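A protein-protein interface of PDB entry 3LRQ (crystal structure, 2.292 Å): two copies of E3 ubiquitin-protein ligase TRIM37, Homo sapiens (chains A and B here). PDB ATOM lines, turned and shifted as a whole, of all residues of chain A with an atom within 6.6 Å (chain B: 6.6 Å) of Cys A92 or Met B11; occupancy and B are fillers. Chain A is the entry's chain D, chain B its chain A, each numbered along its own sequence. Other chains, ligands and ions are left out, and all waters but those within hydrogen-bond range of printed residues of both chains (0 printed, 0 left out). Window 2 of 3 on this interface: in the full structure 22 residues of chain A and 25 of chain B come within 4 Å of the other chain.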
ATOM      1  N   MET A  11      19.299 -27.074  -7.756  1.00  0.00           N
ATOM      2  CA  MET A  11      19.736 -25.954  -8.585  1.00  0.00           C
ATOM      3  C   MET A  11      18.582 -25.414  -9.431  1.00  0.00           C
ATOM      4  O   MET A  11      18.018 -26.125 -10.264  1.00  0.00           O
ATOM      5  CB  MET A  11      20.909 -26.370  -9.485  1.00  0.00           C
ATOM      6  CG  MET A  11      22.018 -25.328  -9.607  1.00  0.00           C
ATOM      7  SD  MET A  11      22.834 -24.895  -7.883  1.00  0.00           S
ATOM      8  CE  MET A  11      23.931 -26.490  -7.634  1.00  0.00           C
ATOM      9  N   GLU A  13      16.632 -24.083 -12.278  1.00  0.00           N
ATOM     10  CA  GLU A  13      16.850 -24.213 -13.711  1.00  0.00           C
ATOM     11  C   GLU A  13      16.906 -22.857 -14.421  1.00  0.00           C
ATOM     12  O   GLU A  13      17.682 -22.671 -15.363  1.00  0.00           O
ATOM     13  CB  GLU A  13      15.753 -25.084 -14.325  1.00  0.00           C
ATOM     14  CG  GLU A  13      16.260 -26.385 -14.920  1.00  0.00           C
ATOM     15  CD  GLU A  13      15.161 -27.423 -15.079  1.00  0.00           C
ATOM     16  OE1 GLU A  13      13.966 -27.052 -15.061  1.00  0.00           O
ATOM     17  OE2 GLU A  13      15.495 -28.618 -15.221  1.00  0.00           O
ATOM     18  N   GLN A  85      31.958 -24.842 -17.619  1.00  0.00           N
ATOM     19  CA  GLN A  85      31.224 -25.047 -16.368  1.00  0.00           C
ATOM     20  C   GLN A  85      29.710 -25.021 -16.560  1.00  0.00           C
ATOM     21  O   GLN A  85      28.990 -25.845 -15.993  1.00  0.00           O
ATOM     22  CB  GLN A  85      31.634 -24.006 -15.321  1.00  0.00           C
ATOM     23  CG  GLN A  85      33.107 -24.031 -14.988  1.00  0.00           C
ATOM     24  CD  GLN A  85      33.535 -25.371 -14.367  1.00  0.00           C
ATOM     25  OE1 GLN A  85      32.697 -26.189 -13.987  1.00  0.00           O
ATOM     26  NE2 GLN A  85      34.840 -25.590 -14.265  1.00  0.00           N
ATOM     27  N   ASP A  87      28.177 -25.878 -19.202  1.00  0.00           N
ATOM     28  CA  ASP A  87      27.861 -27.153 -19.822  1.00  0.00           C
ATOM     29  C   ASP A  87      27.620 -28.220 -18.759  1.00  0.00           C
ATOM     30  O   ASP A  87      26.614 -28.932 -18.793  1.00  0.00           O
ATOM     31  CB  ASP A  87      29.003 -27.573 -20.744  1.00  0.00           C
ATOM     32  CG  ASP A  87      28.597 -28.662 -21.700  1.00  0.00           C
ATOM     33  OD1 ASP A  87      28.537 -29.834 -21.265  1.00  0.00           O
ATOM     34  OD2 ASP A  87      28.335 -28.341 -22.882  1.00  0.00           O
ATOM     35  N   THR A  88      28.545 -28.325 -17.811  1.00  0.00           N
ATOM     36  CA  THR A  88      28.380 -29.241 -16.686  1.00  0.00           C
ATOM     37  C   THR A  88      27.118 -28.940 -15.858  1.00  0.00           C
ATOM     38  O   THR A  88      26.404 -29.849 -15.442  1.00  0.00           O
ATOM     39  CB  THR A  88      29.606 -29.209 -15.756  1.00  0.00           C
ATOM     40  OG1 THR A  88      30.753 -29.702 -16.459  1.00  0.00           O
ATOM     41  CG2 THR A  88      29.362 -30.065 -14.521  1.00  0.00           C
ATOM     42  N   LEU A  89      26.856 -27.662 -15.601  1.00  0.00           N
ATOM     43  CA  LEU A  89      25.653 -27.274 -14.876  1.00  0.00           C
ATOM     44  C   LEU A  89      24.391 -27.725 -15.605  1.00  0.00           C
ATOM     45  O   LEU A  89      23.472 -28.272 -14.997  1.00  0.00           O
ATOM     46  CB  LEU A  89      25.618 -25.764 -14.691  1.00  0.00           C
ATOM     47  CG  LEU A  89      25.978 -25.241 -13.309  1.00  0.00           C
ATOM     48  CD1 LEU A  89      26.006 -23.713 -13.347  1.00  0.00           C
ATOM     49  CD2 LEU A  89      24.969 -25.747 -12.287  1.00  0.00           C
ATOM     50  N   GLN A  90      24.346 -27.484 -16.911  1.00  0.00           N
ATOM     51  CA  GLN A  90      23.181 -27.844 -17.696  1.00  0.00           C
ATOM     52  C   GLN A  90      22.990 -29.363 -17.710  1.00  0.00           C
ATOM     53  O   GLN A  90      21.866 -29.861 -17.694  1.00  0.00           O
ATOM     54  CB  GLN A  90      23.295 -27.264 -19.111  1.00  0.00           C
ATOM     55  CG  GLN A  90      23.793 -25.806 -19.107  1.00  0.00           C
ATOM     56  CD  GLN A  90      22.831 -24.804 -19.747  1.00  0.00           C
ATOM     57  OE1 GLN A  90      21.775 -24.478 -19.187  1.00  0.00           O
ATOM     58  NE2 GLN A  90      23.208 -24.296 -20.920  1.00  0.00           N
ATOM     59  N   LEU A  91      24.098 -30.096 -17.725  1.00  0.00           N
ATOM     60  CA  LEU A  91      24.068 -31.551 -17.650  1.00  0.00           C
ATOM     61  C   LEU A  91      23.392 -31.994 -16.361  1.00  0.00           C
ATOM     62  O   LEU A  91      22.645 -32.971 -16.337  1.00  0.00           O
ATOM     63  CB  LEU A  91      25.495 -32.094 -17.697  1.00  0.00           C
ATOM     64  CG  LEU A  91      25.807 -33.329 -18.543  1.00  0.00           C
ATOM     65  CD1 LEU A  91      24.714 -33.587 -19.570  1.00  0.00           C
ATOM     66  CD2 LEU A  91      27.183 -33.174 -19.217  1.00  0.00           C
ATOM     67  N   CYS A  92      23.653 -31.259 -15.288  1.00  0.00           N
ATOM     68  CA  CYS A  92      23.089 -31.575 -13.979  1.00  0.00           C
ATOM     69  C   CYS A  92      21.563 -31.416 -13.865  1.00  0.00           C
ATOM     70  O   CYS A  92      21.047 -31.122 -12.788  1.00  0.00           O
ATOM     71  CB  CYS A  92      23.800 -30.762 -12.886  1.00  0.00           C
ATOM     72  SG  CYS A  92      25.476 -31.362 -12.502  1.00  0.00           S
ATOM     73  N   SER A  93      20.847 -31.606 -14.973  1.00  0.00           N
ATOM     74  CA  SER A  93      19.394 -31.784 -14.924  1.00  0.00           C
ATOM     75  C   SER A  93      19.102 -33.215 -14.464  1.00  0.00           C
ATOM     76  O   SER A  93      18.189 -33.456 -13.667  1.00  0.00           O
ATOM     77  CB  SER A  93      18.761 -31.525 -16.295  1.00  0.00           C
ATOM     78  N   LEU A  94      19.903 -34.151 -14.972  1.00  0.00           N
ATOM     79  CA  LEU A  94      19.881 -35.553 -14.543  1.00  0.00           C
ATOM     80  C   LEU A  94      18.564 -36.258 -14.828  1.00  0.00           C
ATOM     81  O   LEU A  94      18.374 -37.405 -14.424  1.00  0.00           O
ATOM     82  CB  LEU A  94      20.227 -35.680 -13.054  1.00  0.00           C
ATOM     83  CG  LEU A  94      21.710 -35.832 -12.696  1.00  0.00           C
ATOM     84  CD1 LEU A  94      22.231 -34.627 -11.917  1.00  0.00           C
ATOM     85  CD2 LEU A  94      21.942 -37.117 -11.920  1.00  0.00           C
ATOM     86  N   HIS B  10      26.925 -32.484  -5.341  1.00  0.00           N
ATOM     87  CA  HIS B  10      28.110 -31.709  -4.991  1.00  0.00           C
ATOM     88  C   HIS B  10      28.980 -31.396  -6.210  1.00  0.00           C
ATOM     89  O   HIS B  10      30.056 -30.817  -6.078  1.00  0.00           O
ATOM     90  CB  HIS B  10      28.923 -32.425  -3.908  1.00  0.00           C
ATOM     91  CG  HIS B  10      30.302 -31.869  -3.713  1.00  0.00           C
ATOM     92  ND1 HIS B  10      31.441 -32.572  -4.048  1.00  0.00           N
ATOM     93  CD2 HIS B  10      30.726 -30.677  -3.230  1.00  0.00           C
ATOM     94  CE1 HIS B  10      32.505 -31.839  -3.772  1.00  0.00           C
ATOM     95  NE2 HIS B  10      32.099 -30.684  -3.276  1.00  0.00           N
ATOM     96  N   MET B  11      28.514 -31.768  -7.398  1.00  0.00           N
ATOM     97  CA  MET B  11      29.264 -31.469  -8.619  1.00  0.00           C
ATOM     98  C   MET B  11      28.692 -30.249  -9.336  1.00  0.00           C
ATOM     99  O   MET B  11      29.435 -29.423  -9.860  1.00  0.00           O
ATOM    100  CB  MET B  11      29.342 -32.695  -9.534  1.00  0.00           C
ATOM    101  CG  MET B  11      28.613 -32.597 -10.867  1.00  0.00           C
ATOM    102  SD  MET B  11      28.630 -34.342 -11.773  1.00  0.00           S
ATOM    103  CE  MET B  11      27.840 -35.405 -10.330  1.00  0.00           C
ATOM    104  N   ASP B  12      27.370 -30.136  -9.347  1.00  0.00           N
ATOM    105  CA  ASP B  12      26.733 -28.894  -9.747  1.00  0.00           C
ATOM    106  C   ASP B  12      27.219 -27.765  -8.828  1.00  0.00           C
ATOM    107  O   ASP B  12      27.462 -26.647  -9.277  1.00  0.00           O
ATOM    108  CB  ASP B  12      25.199 -29.025  -9.747  1.00  0.00           C
ATOM    109  CG  ASP B  12      24.640 -29.640  -8.460  1.00  0.00           C
ATOM    110  OD1 ASP B  12      23.422 -29.934  -8.425  1.00  0.00           O
ATOM    111  OD2 ASP B  12      25.402 -29.834  -7.488  1.00  0.00           O
ATOM    112  N   GLU B  13      27.392 -28.088  -7.549  1.00  0.00           N
ATOM    113  CA  GLU B  13      27.915 -27.163  -6.546  1.00  0.00           C
ATOM    114  C   GLU B  13      29.273 -26.593  -6.920  1.00  0.00           C
ATOM    115  O   GLU B  13      29.519 -25.387  -6.778  1.00  0.00           O
ATOM    116  CB  GLU B  13      28.094 -27.880  -5.215  1.00  0.00           C
ATOM    117  CG  GLU B  13      26.924 -27.826  -4.260  1.00  0.00           C
ATOM    118  CD  GLU B  13      27.306 -28.395  -2.899  1.00  0.00           C
ATOM    119  OE1 GLU B  13      28.524 -28.433  -2.597  1.00  0.00           O
ATOM    120  OE2 GLU B  13      26.404 -28.805  -2.138  1.00  0.00           O
ATOM    121  N   GLN B  14      30.173 -27.468  -7.352  1.00  0.00           N
ATOM    122  CA  GLN B  14      31.521 -27.038  -7.652  1.00  0.00           C
ATOM    123  C   GLN B  14      31.579 -26.319  -8.995  1.00  0.00           C
ATOM    124  O   GLN B  14      32.490 -25.534  -9.239  1.00  0.00           O
ATOM    125  CB  GLN B  14      32.494 -28.220  -7.605  1.00  0.00           C
ATOM    126  CG  GLN B  14      32.171 -29.349  -8.572  1.00  0.00           C
ATOM    127  CD  GLN B  14      32.690 -30.707  -8.096  1.00  0.00           C
ATOM    128  OE1 GLN B  14      32.702 -30.997  -6.898  1.00  0.00           O
ATOM    129  NE2 GLN B  14      33.116 -31.544  -9.039  1.00  0.00           N
ATOM    130  N   SER B  15      30.619 -26.593  -9.873  1.00  0.00           N
ATOM    131  CA  SER B  15      30.538 -25.836 -11.119  1.00  0.00           C
ATOM    132  C   SER B  15      30.130 -24.393 -10.822  1.00  0.00           C
ATOM    133  O   SER B  15      30.749 -23.461 -11.317  1.00  0.00           O
ATOM    134  CB  SER B  15      29.572 -26.478 -12.111  1.00  0.00           C
ATOM    135  OG  SER B  15      30.235 -27.454 -12.887  1.00  0.00           O
ATOM    136  N   VAL B  16      29.098 -24.215 -10.000  1.00  0.00           N
ATOM    137  CA  VAL B  16      28.700 -22.884  -9.589  1.00  0.00           C
ATOM    138  C   VAL B  16      29.889 -22.137  -8.992  1.00  0.00           C
ATOM    139  O   VAL B  16      30.133 -20.977  -9.323  1.00  0.00           O
ATOM    140  CB  VAL B  16      27.585 -22.927  -8.541  1.00  0.00           C
ATOM    141  CG1 VAL B  16      27.501 -21.590  -7.809  1.00  0.00           C
ATOM    142  CG2 VAL B  16      26.242 -23.299  -9.195  1.00  0.00           C
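Of the 11 printed residues of chain A, 5 touch a printed residue of chain B.
Of the 7 printed residues of chain B, 5 touch a printed residue of chain A.
Printed residues of chain B that touch a printed residue of chain A: Met B11, Asp B12, Glu B13, Ser B15 and Val B16.
Hydrophobic or aromatic side chains of chain B within 4 Å of the printed part of chain A: Met B11 and Val B16.
Among the printed residues, 8 pairs touch across the chains.
Among the printed residues, merely in contact across the chains: Thr A88 with Ser B15 (3.2 Å), Met A11 with Asp B12 (3.3 Å), Cys A92 with Asp B12 (3.6 Å), Cys A92 with Met B11 (3.7 Å), Met A11 with Glu B13 (3.8 Å), Leu A89 with Ser B15 (3.99 Å) and Met A11 with Val B16 (3.99 Å).
Met A11 touches Glu B13, but with the chains exchanged Glu A13 does not touch Met B11 (13.9 Å).
Of the 8 pairs that touch across the chains among the printed residues, none has its exchanged pair printed and touching as well.
The backbone carbonyl oxygen (O) of Thr A88 lies within hydrogen-bond range of the side-chain sulfur (SG) of Cys A92 (3.4 Å).
Printed residues of chain A within 4 Å of Met B11: Cys A92.
Of the printed residues of chain A, Val B16 touches Met A11 (3.99 Å).
Of the printed residues of chain B, Met A11 touches Asp B12, Glu B13 and Val B16.
Of the printed residues of chain A, Asp B12 touches Met A11 and Cys A92.
Gln B14 touches none of the printed residues of chain A.
Leu A94 touches none of the printed residues of chain B.
The nearest residue of chain B that does not touch Cys A92 is Ser B15 (6.2 Å).
The nearest residue of chain A that does not touch Met B11 is Thr A88 (4.5 Å).
OG of Ser B15 is in hydrogen-bond range of OE1 of Gln A85.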
